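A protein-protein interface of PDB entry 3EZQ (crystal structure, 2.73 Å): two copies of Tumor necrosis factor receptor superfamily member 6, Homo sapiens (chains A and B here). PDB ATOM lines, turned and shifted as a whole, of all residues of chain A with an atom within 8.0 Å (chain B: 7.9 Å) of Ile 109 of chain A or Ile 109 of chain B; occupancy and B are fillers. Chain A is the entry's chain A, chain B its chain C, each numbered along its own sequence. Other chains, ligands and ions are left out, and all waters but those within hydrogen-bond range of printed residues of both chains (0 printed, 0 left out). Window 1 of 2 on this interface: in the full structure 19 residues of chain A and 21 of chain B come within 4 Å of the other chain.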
ATOM      1  N   LEU A  84      10.279  20.009 -21.297  1.00  0.00           N
ATOM      2  CA  LEU A  84      11.142  21.097 -21.741  1.00  0.00           C
ATOM      3  C   LEU A  84      12.232  21.397 -20.719  1.00  0.00           C
ATOM      4  O   LEU A  84      13.388  21.564 -21.068  1.00  0.00           O
ATOM      5  CB  LEU A  84      10.333  22.355 -21.921  1.00  0.00           C
ATOM      6  CG  LEU A  84       9.690  22.559 -23.274  1.00  0.00           C
ATOM      7  CD1 LEU A  84       8.602  23.604 -23.098  1.00  0.00           C
ATOM      8  CD2 LEU A  84      10.730  23.000 -24.288  1.00  0.00           C
ATOM      9  N   LYS A  87      14.811  18.556 -20.827  1.00  0.00           N
ATOM     10  CA  LYS A  87      15.585  18.545 -22.021  1.00  0.00           C
ATOM     11  C   LYS A  87      16.493  19.760 -22.144  1.00  0.00           C
ATOM     12  O   LYS A  87      17.644  19.614 -22.573  1.00  0.00           O
ATOM     13  CB  LYS A  87      14.666  18.354 -23.202  1.00  0.00           C
ATOM     14  CG  LYS A  87      14.258  16.890 -23.300  1.00  0.00           C
ATOM     15  CD  LYS A  87      13.339  16.668 -24.470  1.00  0.00           C
ATOM     16  CE  LYS A  87      12.810  15.265 -24.509  1.00  0.00           C
ATOM     17  NZ  LYS A  87      13.895  14.210 -24.487  1.00  0.00           N
ATOM     18  N   ILE A  88      16.024  20.934 -21.720  1.00  0.00           N
ATOM     19  CA  ILE A  88      16.862  22.115 -21.769  1.00  0.00           C
ATOM     20  C   ILE A  88      17.955  22.026 -20.710  1.00  0.00           C
ATOM     21  O   ILE A  88      19.115  22.373 -20.976  1.00  0.00           O
ATOM     22  CB  ILE A  88      16.083  23.431 -21.639  1.00  0.00           C
ATOM     23  CG1 ILE A  88      15.080  23.573 -22.810  1.00  0.00           C
ATOM     24  CG2 ILE A  88      17.066  24.598 -21.621  1.00  0.00           C
ATOM     25  CD1 ILE A  88      13.962  24.616 -22.551  1.00  0.00           C
ATOM     26  N   GLN A  89      17.635  21.501 -19.533  1.00  0.00           N
ATOM     27  CA  GLN A  89      18.701  21.317 -18.541  1.00  0.00           C
ATOM     28  C   GLN A  89      19.810  20.415 -19.037  1.00  0.00           C
ATOM     29  O   GLN A  89      20.977  20.680 -18.796  1.00  0.00           O
ATOM     30  CB  GLN A  89      18.180  20.746 -17.261  1.00  0.00           C
ATOM     31  CG  GLN A  89      19.266  20.567 -16.266  1.00  0.00           C
ATOM     32  CD  GLN A  89      18.729  20.310 -14.875  1.00  0.00           C
ATOM     33  OE1 GLN A  89      18.312  19.179 -14.536  1.00  0.00           O
ATOM     34  NE2 GLN A  89      18.726  21.359 -14.060  1.00  0.00           N
ATOM     35  N   ILE A  91      20.789  19.910 -22.191  1.00  0.00           N
ATOM     36  CA  ILE A  91      21.600  20.653 -23.162  1.00  0.00           C
ATOM     37  C   ILE A  91      22.567  21.609 -22.453  1.00  0.00           C
ATOM     38  O   ILE A  91      23.756  21.581 -22.703  1.00  0.00           O
ATOM     39  CB  ILE A  91      20.670  21.434 -24.128  1.00  0.00           C
ATOM     40  CG1 ILE A  91      19.982  20.456 -25.103  1.00  0.00           C
ATOM     41  CG2 ILE A  91      21.457  22.541 -24.870  1.00  0.00           C
ATOM     42  CD1 ILE A  91      18.529  20.837 -25.452  1.00  0.00           C
ATOM     43  N   ILE A  92      22.040  22.400 -21.536  1.00  0.00           N
ATOM     44  CA  ILE A  92      22.830  23.384 -20.804  1.00  0.00           C
ATOM     45  C   ILE A  92      23.975  22.749 -20.020  1.00  0.00           C
ATOM     46  O   ILE A  92      25.120  23.178 -20.178  1.00  0.00           O
ATOM     47  CB  ILE A  92      21.960  24.246 -19.875  1.00  0.00           C
ATOM     48  CG1 ILE A  92      21.021  25.095 -20.747  1.00  0.00           C
ATOM     49  CG2 ILE A  92      22.860  25.073 -18.996  1.00  0.00           C
ATOM     50  CD1 ILE A  92      20.120  26.028 -20.042  1.00  0.00           C
ATOM     51  N   ASP A  95      26.617  21.466 -22.479  1.00  0.00           N
ATOM     52  CA  ASP A  95      27.451  22.541 -23.035  1.00  0.00           C
ATOM     53  C   ASP A  95      28.293  23.325 -22.027  1.00  0.00           C
ATOM     54  O   ASP A  95      29.353  23.782 -22.372  1.00  0.00           O
ATOM     55  CB  ASP A  95      26.601  23.496 -23.865  1.00  0.00           C
ATOM     56  CG  ASP A  95      25.850  22.783 -24.969  1.00  0.00           C
ATOM     57  OD1 ASP A  95      26.289  21.675 -25.388  1.00  0.00           O
ATOM     58  OD2 ASP A  95      24.796  23.314 -25.402  1.00  0.00           O
ATOM     59  N   ASN A 104      25.737  24.505 -31.680  1.00  0.00           N
ATOM     60  CA  ASN A 104      24.447  23.837 -31.862  1.00  0.00           C
ATOM     61  C   ASN A 104      23.384  24.246 -30.812  1.00  0.00           C
ATOM     62  O   ASN A 104      22.192  23.912 -30.953  1.00  0.00           O
ATOM     63  CB  ASN A 104      24.636  22.295 -31.906  1.00  0.00           C
ATOM     64  CG  ASN A 104      25.595  21.757 -30.801  1.00  0.00           C
ATOM     65  OD1 ASN A 104      25.459  22.109 -29.620  1.00  0.00           O
ATOM     66  ND2 ASN A 104      26.550  20.898 -31.190  1.00  0.00           N
ATOM     67  N   PHE A 105      23.789  24.966 -29.767  1.00  0.00           N
ATOM     68  CA  PHE A 105      22.846  25.287 -28.687  1.00  0.00           C
ATOM     69  C   PHE A 105      21.543  25.966 -29.169  1.00  0.00           C
ATOM     70  O   PHE A 105      20.460  25.580 -28.784  1.00  0.00           O
ATOM     71  CB  PHE A 105      23.487  26.151 -27.585  1.00  0.00           C
ATOM     72  CG  PHE A 105      22.520  26.498 -26.521  1.00  0.00           C
ATOM     73  CD1 PHE A 105      22.253  25.596 -25.504  1.00  0.00           C
ATOM     74  CD2 PHE A 105      21.762  27.657 -26.601  1.00  0.00           C
ATOM     75  CE1 PHE A 105      21.267  25.872 -24.518  1.00  0.00           C
ATOM     76  CE2 PHE A 105      20.774  27.942 -25.644  1.00  0.00           C
ATOM     77  CZ  PHE A 105      20.520  27.042 -24.597  1.00  0.00           C
ATOM     78  N   ARG A 106      21.671  27.013 -29.968  1.00  0.00           N
ATOM     79  CA  ARG A 106      20.522  27.726 -30.495  1.00  0.00           C
ATOM     80  C   ARG A 106      19.625  26.799 -31.308  1.00  0.00           C
ATOM     81  O   ARG A 106      18.420  26.814 -31.158  1.00  0.00           O
ATOM     82  CB  ARG A 106      21.014  28.903 -31.355  1.00  0.00           C
ATOM     83  CG  ARG A 106      19.969  29.535 -32.266  1.00  0.00           C
ATOM     84  CD  ARG A 106      20.533  30.724 -33.012  1.00  0.00           C
ATOM     85  NE  ARG A 106      19.492  31.424 -33.761  1.00  0.00           N
ATOM     86  CZ  ARG A 106      19.258  31.277 -35.066  1.00  0.00           C
ATOM     87  NH1 ARG A 106      19.976  30.440 -35.805  1.00  0.00           N
ATOM     88  NH2 ARG A 106      18.283  31.976 -35.635  1.00  0.00           N
ATOM     89  N   ASN A 107      20.224  26.006 -32.189  1.00  0.00           N
ATOM     90  CA  ASN A 107      19.473  25.058 -33.017  1.00  0.00           C
ATOM     91  C   ASN A 107      18.766  24.077 -32.132  1.00  0.00           C
ATOM     92  O   ASN A 107      17.611  23.762 -32.350  1.00  0.00           O
ATOM     93  CB  ASN A 107      20.381  24.223 -33.921  1.00  0.00           C
ATOM     94  CG  ASN A 107      21.244  25.053 -34.810  1.00  0.00           C
ATOM     95  OD1 ASN A 107      20.759  25.683 -35.746  1.00  0.00           O
ATOM     96  ND2 ASN A 107      22.550  25.045 -34.543  1.00  0.00           N
ATOM     97  N   GLU A 108      19.480  23.570 -31.140  1.00  0.00           N
ATOM     98  CA  GLU A 108      18.895  22.605 -30.240  1.00  0.00           C
ATOM     99  C   GLU A 108      17.658  23.167 -29.565  1.00  0.00           C
ATOM    100  O   GLU A 108      16.581  22.567 -29.654  1.00  0.00           O
ATOM    101  CB  GLU A 108      19.909  22.118 -29.225  1.00  0.00           C
ATOM    102  CG  GLU A 108      20.889  21.148 -29.832  1.00  0.00           C
ATOM    103  CD  GLU A 108      22.126  20.913 -28.994  1.00  0.00           C
ATOM    104  OE1 GLU A 108      23.128  20.379 -29.541  1.00  0.00           O
ATOM    105  OE2 GLU A 108      22.109  21.259 -27.796  1.00  0.00           O
ATOM    106  N   ILE A 109      17.781  24.328 -28.922  1.00  0.00           N
ATOM    107  CA  ILE A 109      16.626  24.940 -28.290  1.00  0.00           C
ATOM    108  C   ILE A 109      15.515  25.173 -29.300  1.00  0.00           C
ATOM    109  O   ILE A 109      14.379  24.874 -29.004  1.00  0.00           O
ATOM    110  CB  ILE A 109      16.984  26.249 -27.542  1.00  0.00           C
ATOM    111  CG1 ILE A 109      17.693  25.910 -26.247  1.00  0.00           C
ATOM    112  CG2 ILE A 109      15.722  27.040 -27.122  1.00  0.00           C
ATOM    113  CD1 ILE A 109      16.730  25.334 -25.265  1.00  0.00           C
ATOM    114  N   GLN A 110      15.830  25.692 -30.478  1.00  0.00           N
ATOM    115  CA  GLN A 110      14.785  26.032 -31.438  1.00  0.00           C
ATOM    116  C   GLN A 110      13.977  24.819 -31.864  1.00  0.00           C
ATOM    117  O   GLN A 110      12.776  24.927 -32.079  1.00  0.00           O
ATOM    118  CB  GLN A 110      15.363  26.773 -32.655  1.00  0.00           C
ATOM    119  CG  GLN A 110      15.838  28.216 -32.330  1.00  0.00           C
ATOM    120  CD  GLN A 110      15.815  29.157 -33.515  1.00  0.00           C
ATOM    121  OE1 GLN A 110      14.840  29.195 -34.260  1.00  0.00           O
ATOM    122  NE2 GLN A 110      16.892  29.912 -33.705  1.00  0.00           N
ATOM    123  N   SER A 111      14.624  23.664 -31.976  1.00  0.00           N
ATOM    124  CA  SER A 111      13.924  22.453 -32.388  1.00  0.00           C
ATOM    125  C   SER A 111      12.941  21.986 -31.325  1.00  0.00           C
ATOM    126  O   SER A 111      11.913  21.409 -31.663  1.00  0.00           O
ATOM    127  CB  SER A 111      14.903  21.341 -32.765  1.00  0.00           C
ATOM    128  OG  SER A 111      15.456  20.759 -31.608  1.00  0.00           O
ATOM    129  N   LEU A 112      13.233  22.244 -30.053  1.00  0.00           N
ATOM    130  CA  LEU A 112      12.346  21.827 -28.964  1.00  0.00           C
ATOM    131  C   LEU A 112      11.036  22.610 -28.987  1.00  0.00           C
ATOM    132  O   LEU A 112      10.042  22.176 -28.421  1.00  0.00           O
ATOM    133  CB  LEU A 112      13.008  22.027 -27.587  1.00  0.00           C
ATOM    134  CG  LEU A 112      14.146  21.054 -27.249  1.00  0.00           C
ATOM    135  CD1 LEU A 112      14.803  21.424 -25.948  1.00  0.00           C
ATOM    136  CD2 LEU A 112      13.645  19.587 -27.214  1.00  0.00           C
ATOM    137  N   VAL A 113      11.027  23.764 -29.645  1.00  0.00           N
ATOM    138  CA  VAL A 113       9.828  24.622 -29.663  1.00  0.00           C
ATOM    139  C   VAL A 113       9.317  24.867 -31.098  1.00  0.00           C
ATOM    140  O   VAL A 113       8.613  25.839 -31.376  1.00  0.00           O
ATOM    141  CB  VAL A 113       9.994  26.012 -28.971  1.00  0.00           C
ATOM    142  CG1 VAL A 113      10.380  25.845 -27.512  1.00  0.00           C
ATOM    143  CG2 VAL A 113      10.948  26.895 -29.738  1.00  0.00           C
ATOM    144  N   LEU A 114       9.660  23.969 -31.999  1.00  0.00           N
ATOM    145  CA  LEU A 114       9.272  24.084 -33.393  1.00  0.00           C
ATOM    146  C   LEU A 114       7.756  24.144 -33.566  1.00  0.00           C
ATOM    147  O   LEU A 114       7.032  23.355 -32.976  1.00  0.00           O
ATOM    148  CB  LEU A 114       9.801  22.868 -34.154  1.00  0.00           C
ATOM    149  CG  LEU A 114       9.953  23.054 -35.648  1.00  0.00           C
ATOM    150  CD1 LEU A 114      11.331  23.657 -35.921  1.00  0.00           C
ATOM    151  CD2 LEU A 114       9.773  21.726 -36.354  1.00  0.00           C
ATOM    152  N   LEU B  84      21.169  32.005 -19.717  1.00  0.00           N
ATOM    153  CA  LEU B  84      20.064  31.245 -20.336  1.00  0.00           C
ATOM    154  C   LEU B  84      19.346  30.366 -19.302  1.00  0.00           C
ATOM    155  O   LEU B  84      18.123  30.370 -19.214  1.00  0.00           O
ATOM    156  CB  LEU B  84      20.563  30.401 -21.495  1.00  0.00           C
ATOM    157  CG  LEU B  84      20.665  31.163 -22.807  1.00  0.00           C
ATOM    158  CD1 LEU B  84      21.627  30.463 -23.755  1.00  0.00           C
ATOM    159  CD2 LEU B  84      19.303  31.322 -23.416  1.00  0.00           C
ATOM    160  N   LYS B  87      17.247  32.490 -17.083  1.00  0.00           N
ATOM    161  CA  LYS B  87      16.125  33.127 -17.738  1.00  0.00           C
ATOM    162  C   LYS B  87      15.100  32.137 -18.165  1.00  0.00           C
ATOM    163  O   LYS B  87      13.924  32.367 -17.963  1.00  0.00           O
ATOM    164  CB  LYS B  87      16.570  34.026 -18.891  1.00  0.00           C
ATOM    165  CG  LYS B  87      17.093  35.395 -18.374  1.00  0.00           C
ATOM    166  CD  LYS B  87      17.325  36.467 -19.455  1.00  0.00           C
ATOM    167  CE  LYS B  87      17.639  37.852 -18.831  1.00  0.00           C
ATOM    168  NZ  LYS B  87      16.690  38.337 -17.702  1.00  0.00           N
ATOM    169  N   ILE B  88      15.521  30.984 -18.695  1.00  0.00           N
ATOM    170  CA  ILE B  88      14.527  29.966 -19.064  1.00  0.00           C
ATOM    171  C   ILE B  88      13.862  29.378 -17.826  1.00  0.00           C
ATOM    172  O   ILE B  88      12.648  29.182 -17.793  1.00  0.00           O
ATOM    173  CB  ILE B  88      15.073  28.888 -19.916  1.00  0.00           C
ATOM    174  CG1 ILE B  88      15.541  29.481 -21.244  1.00  0.00           C
ATOM    175  CG2 ILE B  88      13.995  27.820 -20.122  1.00  0.00           C
ATOM    176  CD1 ILE B  88      16.619  28.616 -21.965  1.00  0.00           C
ATOM    177  N   GLN B  89      14.621  29.148 -16.773  1.00  0.00           N
ATOM    178  CA  GLN B  89      13.991  28.663 -15.565  1.00  0.00           C
ATOM    179  C   GLN B  89      12.868  29.574 -15.104  1.00  0.00           C
ATOM    180  O   GLN B  89      11.838  29.100 -14.668  1.00  0.00           O
ATOM    181  CB  GLN B  89      15.005  28.504 -14.454  1.00  0.00           C
ATOM    182  CG  GLN B  89      14.326  28.311 -13.109  1.00  0.00           C
ATOM    183  CD  GLN B  89      15.220  27.667 -12.108  1.00  0.00           C
ATOM    184  OE1 GLN B  89      15.998  28.358 -11.472  1.00  0.00           O
ATOM    185  NE2 GLN B  89      15.115  26.357 -11.943  1.00  0.00           N
ATOM    186  N   ILE B  91      10.983  31.670 -16.901  1.00  0.00           N
ATOM    187  CA  ILE B  91       9.801  31.562 -17.776  1.00  0.00           C
ATOM    188  C   ILE B  91       9.024  30.283 -17.404  1.00  0.00           C
ATOM    189  O   ILE B  91       7.792  30.337 -17.186  1.00  0.00           O
ATOM    190  CB  ILE B  91      10.163  31.499 -19.244  1.00  0.00           C
ATOM    191  CG1 ILE B  91      10.590  32.877 -19.719  1.00  0.00           C
ATOM    192  CG2 ILE B  91       8.994  30.976 -20.065  1.00  0.00           C
ATOM    193  CD1 ILE B  91      11.548  32.837 -20.850  1.00  0.00           C
ATOM    194  N   ILE B  92       9.740  29.148 -17.322  1.00  0.00           N
ATOM    195  CA  ILE B  92       9.085  27.857 -17.073  1.00  0.00           C
ATOM    196  C   ILE B  92       8.358  27.809 -15.750  1.00  0.00           C
ATOM    197  O   ILE B  92       7.199  27.408 -15.716  1.00  0.00           O
ATOM    198  CB  ILE B  92      10.055  26.627 -17.159  1.00  0.00           C
ATOM    199  CG1 ILE B  92      10.513  26.417 -18.600  1.00  0.00           C
ATOM    200  CG2 ILE B  92       9.378  25.334 -16.647  1.00  0.00           C
ATOM    201  CD1 ILE B  92      11.586  25.484 -18.725  1.00  0.00           C
ATOM    202  N   ASP B  95       5.265  30.086 -16.045  1.00  0.00           N
ATOM    203  CA  ASP B  95       4.188  29.444 -16.794  1.00  0.00           C
ATOM    204  C   ASP B  95       3.601  28.231 -16.121  1.00  0.00           C
ATOM    205  O   ASP B  95       2.411  27.971 -16.252  1.00  0.00           O
ATOM    206  CB  ASP B  95       4.644  29.043 -18.190  1.00  0.00           C
ATOM    207  CG  ASP B  95       4.860  30.233 -19.067  1.00  0.00           C
ATOM    208  OD1 ASP B  95       4.713  31.367 -18.529  1.00  0.00           O
ATOM    209  OD2 ASP B  95       5.163  30.052 -20.276  1.00  0.00           O
ATOM    210  N   ASN B 104       2.872  32.819 -25.172  1.00  0.00           N
ATOM    211  CA  ASN B 104       4.110  33.558 -25.348  1.00  0.00           C
ATOM    212  C   ASN B 104       5.393  32.714 -25.170  1.00  0.00           C
ATOM    213  O   ASN B 104       6.506  33.161 -25.534  1.00  0.00           O
ATOM    214  CB  ASN B 104       4.190  34.712 -24.348  1.00  0.00           C
ATOM    215  CG  ASN B 104       3.050  35.698 -24.503  1.00  0.00           C
ATOM    216  OD1 ASN B 104       2.646  36.024 -25.617  1.00  0.00           O
ATOM    217  ND2 ASN B 104       2.528  36.176 -23.380  1.00  0.00           N
ATOM    218  N   PHE B 105       5.255  31.510 -24.605  1.00  0.00           N
ATOM    219  CA  PHE B 105       6.433  30.723 -24.249  1.00  0.00           C
ATOM    220  C   PHE B 105       7.434  30.542 -25.399  1.00  0.00           C
ATOM    221  O   PHE B 105       8.631  30.825 -25.229  1.00  0.00           O
ATOM    222  CB  PHE B 105       6.051  29.355 -23.717  1.00  0.00           C
ATOM    223  CG  PHE B 105       7.227  28.526 -23.417  1.00  0.00           C
ATOM    224  CD1 PHE B 105       7.871  28.657 -22.213  1.00  0.00           C
ATOM    225  CD2 PHE B 105       7.750  27.670 -24.373  1.00  0.00           C
ATOM    226  CE1 PHE B 105       9.012  27.913 -21.935  1.00  0.00           C
ATOM    227  CE2 PHE B 105       8.900  26.924 -24.111  1.00  0.00           C
ATOM    228  CZ  PHE B 105       9.535  27.048 -22.885  1.00  0.00           C
ATOM    229  N   ARG B 106       6.948  30.060 -26.548  1.00  0.00           N
ATOM    230  CA  ARG B 106       7.799  29.840 -27.706  1.00  0.00           C
ATOM    231  C   ARG B 106       8.515  31.117 -28.095  1.00  0.00           C
ATOM    232  O   ARG B 106       9.729  31.120 -28.306  1.00  0.00           O
ATOM    233  CB  ARG B 106       6.995  29.361 -28.904  1.00  0.00           C
ATOM    234  CG  ARG B 106       7.847  29.059 -30.150  1.00  0.00           C
ATOM    235  CD  ARG B 106       7.028  29.122 -31.430  1.00  0.00           C
ATOM    236  NE  ARG B 106       7.859  29.020 -32.630  1.00  0.00           N
ATOM    237  CZ  ARG B 106       7.439  29.296 -33.869  1.00  0.00           C
ATOM    238  NH1 ARG B 106       6.183  29.687 -34.100  1.00  0.00           N
ATOM    239  NH2 ARG B 106       8.275  29.171 -34.900  1.00  0.00           N
ATOM    240  N   ASN B 107       7.766  32.211 -28.184  1.00  0.00           N
ATOM    241  CA  ASN B 107       8.343  33.493 -28.578  1.00  0.00           C
ATOM    242  C   ASN B 107       9.395  33.902 -27.561  1.00  0.00           C
ATOM    243  O   ASN B 107      10.478  34.363 -27.930  1.00  0.00           O
ATOM    244  CB  ASN B 107       7.249  34.543 -28.752  1.00  0.00           C
ATOM    245  CG  ASN B 107       6.264  34.167 -29.855  1.00  0.00           C
ATOM    246  OD1 ASN B 107       6.572  34.264 -31.048  1.00  0.00           O
ATOM    247  ND2 ASN B 107       5.058  33.788 -29.459  1.00  0.00           N
ATOM    248  N   GLU B 108       9.089  33.689 -26.284  1.00  0.00           N
ATOM    249  CA  GLU B 108      10.026  34.032 -25.230  1.00  0.00           C
ATOM    250  C   GLU B 108      11.327  33.296 -25.447  1.00  0.00           C
ATOM    251  O   GLU B 108      12.382  33.924 -25.617  1.00  0.00           O
ATOM    252  CB  GLU B 108       9.417  33.749 -23.857  1.00  0.00           C
ATOM    253  CG  GLU B 108       8.513  34.921 -23.349  1.00  0.00           C
ATOM    254  CD  GLU B 108       7.294  34.493 -22.515  1.00  0.00           C
ATOM    255  OE1 GLU B 108       6.385  35.334 -22.321  1.00  0.00           O
ATOM    256  OE2 GLU B 108       7.224  33.332 -22.048  1.00  0.00           O
ATOM    257  N   ILE B 109      11.260  31.973 -25.522  1.00  0.00           N
ATOM    258  CA  ILE B 109      12.466  31.171 -25.764  1.00  0.00           C
ATOM    259  C   ILE B 109      13.190  31.611 -27.035  1.00  0.00           C
ATOM    260  O   ILE B 109      14.398  31.798 -27.025  1.00  0.00           O
ATOM    261  CB  ILE B 109      12.142  29.666 -25.868  1.00  0.00           C
ATOM    262  CG1 ILE B 109      11.627  29.150 -24.538  1.00  0.00           C
ATOM    263  CG2 ILE B 109      13.368  28.861 -26.232  1.00  0.00           C
ATOM    264  CD1 ILE B 109      12.580  29.346 -23.465  1.00  0.00           C
ATOM    265  N   GLN B 110      12.454  31.817 -28.115  1.00  0.00           N
ATOM    266  CA  GLN B 110      13.074  32.198 -29.373  1.00  0.00           C
ATOM    267  C   GLN B 110      13.887  33.486 -29.269  1.00  0.00           C
ATOM    268  O   GLN B 110      14.979  33.570 -29.845  1.00  0.00           O
ATOM    269  CB  GLN B 110      12.000  32.378 -30.436  1.00  0.00           C
ATOM    270  CG  GLN B 110      11.164  31.119 -30.731  1.00  0.00           C
ATOM    271  CD  GLN B 110      11.552  30.482 -32.030  1.00  0.00           C
ATOM    272  OE1 GLN B 110      12.738  30.218 -32.258  1.00  0.00           O
ATOM    273  NE2 GLN B 110      10.569  30.236 -32.904  1.00  0.00           N
ATOM    274  N   SER B 111      13.375  34.481 -28.536  1.00  0.00           N
ATOM    275  CA  SER B 111      14.085  35.766 -28.368  1.00  0.00           C
ATOM    276  C   SER B 111      15.411  35.594 -27.670  1.00  0.00           C
ATOM    277  O   SER B 111      16.351  36.355 -27.932  1.00  0.00           O
ATOM    278  CB  SER B 111      13.284  36.771 -27.530  1.00  0.00           C
ATOM    279  OG  SER B 111      11.904  36.485 -27.537  1.00  0.00           O
ATOM    280  N   LEU B 112      15.479  34.627 -26.753  1.00  0.00           N
ATOM    281  CA  LEU B 112      16.683  34.438 -25.944  1.00  0.00           C
ATOM    282  C   LEU B 112      17.834  33.944 -26.787  1.00  0.00           C
ATOM    283  O   LEU B 112      18.997  34.103 -26.435  1.00  0.00           O
ATOM    284  CB  LEU B 112      16.395  33.492 -24.781  1.00  0.00           C
ATOM    285  CG  LEU B 112      15.425  34.138 -23.779  1.00  0.00           C
ATOM    286  CD1 LEU B 112      14.860  33.132 -22.782  1.00  0.00           C
ATOM    287  CD2 LEU B 112      16.123  35.309 -23.092  1.00  0.00           C
ATOM    288  N   VAL B 113      17.499  33.420 -27.947  1.00  0.00           N
ATOM    289  CA  VAL B 113      18.431  32.698 -28.769  1.00  0.00           C
ATOM    290  C   VAL B 113      18.553  33.341 -30.177  1.00  0.00           C
ATOM    291  O   VAL B 113      19.110  32.764 -31.111  1.00  0.00           O
ATOM    292  CB  VAL B 113      17.904  31.227 -28.751  1.00  0.00           C
ATOM    293  CG1 VAL B 113      17.641  30.689 -30.113  1.00  0.00           C
ATOM    294  CG2 VAL B 113      18.800  30.336 -27.895  1.00  0.00           C
ATOM    295  N   LEU B 114      18.071  34.573 -30.302  1.00  0.00           N
ATOM    296  CA  LEU B 114      18.004  35.275 -31.581  1.00  0.00           C
ATOM    297  C   LEU B 114      19.365  35.458 -32.262  1.00  0.00           C
ATOM    298  O   LEU B 114      20.324  35.887 -31.641  1.00  0.00           O
ATOM    299  CB  LEU B 114      17.353  36.639 -31.362  1.00  0.00           C
ATOM    300  CG  LEU B 114      16.653  37.192 -32.602  1.00  0.00           C
ATOM    301  CD1 LEU B 114      15.141  37.315 -32.310  1.00  0.00           C
ATOM    302  CD2 LEU B 114      17.300  38.518 -33.092  1.00  0.00           C
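The guanidinium group (NE) of Arg 106 of chain A is in hydrogen-bond range of the backbone carbonyl oxygen (O) of Val 113 of chain B.
OE1 of Gln 110 of chain A lies close to OE1 of Gln 110 of chain B (3.1 Å).
CD1 of Leu 84 of chain A touches CE2 of Phe 105 of chain B, 3.5 Å away.
CE2 of Phe 105 of chain A touches CD1 of Leu 84 of chain B (3.3 Å).
CE2 of Phe 105 of chain A touches CG2 of Val 113 of chain B, at 3.8 Å.
Ile 109 of chain A touches Ile 109 of chain B (CG2 to CG2, 3.1 Å).
Gln 110 of chain A touches Val 113 of chain B.
Phe 105 of chain B touches Val 113 of chain A.
NE of Arg 106 of chain B touches O of Val 113 of chain A, 3.5 Å away.
NE2 of Gln 110 of chain A sits close to NE of Arg 106 of chain A, 3.0 Å away.
The side-chain amide nitrogen (NE2) of Gln 110 of chain B sits close to the guanidinium group (NE) of Arg 106 of chain B, 3.0 Å away.
Hydrophobic or aromatic side chains of chain A that line the printed part of chain B: Leu 84, Phe 105, Ile 109 and Val 113.
Of the 18 printed residues of chain B, 6 touch a printed residue of chain A.
Among the printed residues, 9 pairs touch across the chains.
Among the printed residues, no Asp or Glu carboxylate lies within 4 Å of a Lys or Arg side-chain nitrogen of the other chain.
Leu 84 of chain A touches Phe 105 of chain B, and with the chains exchanged Phe 105 of chain A touches Leu 84 of chain B.
Phe 105 of chain A touches Val 113 of chain B, and with the chains exchanged Val 113 of chain A touches Phe 105 of chain B.
Arg 106 of chain A touches Val 113 of chain B, and with the chains exchanged Val 113 of chain A touches Arg 106 of chain B.
Gln 110 of chain A touches its own counterpart, Gln 110 of chain B.
Positions printed for both chains: 84, 87, 88, 89, 91, 92, 95, 104, 105, 106, 107, 108, 109, 110, 111, 112, 113 and 114.
Of the 9 pairs that touch across the chains among the printed residues, 8 have their exchanged pair printed and touching as well.
Ile 109 of chain A touches just one residue of chain B: Ile 109 (3.1 Å).
Of chain A, only Ile 109 (3.1 Å) comes within 4 Å of Ile 109 of chain B.
Of the printed residues of chain A, Arg 106 of chain B touches Val 113 (3.5 Å).
Of the printed residues of chain A, Phe 105 of chain B touches Leu 84 (3.5 Å) and Val 113 (3.9 Å).
Of the printed residues of chain A, Val 113 of chain B touches Phe 105, Arg 106 and Gln 110.
Printed residues of chain B within 4 Å of Val 113 of chain A: Phe 105 (3.9 Å) and Arg 106 (3.5 Å).
Of the printed residues of chain A, Gln 110 of chain B touches Gln 110 (3.1 Å).
The nearest residue of chain B that does not touch Ile 109 of chain A is Val 113 of chain B (4.5 Å).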
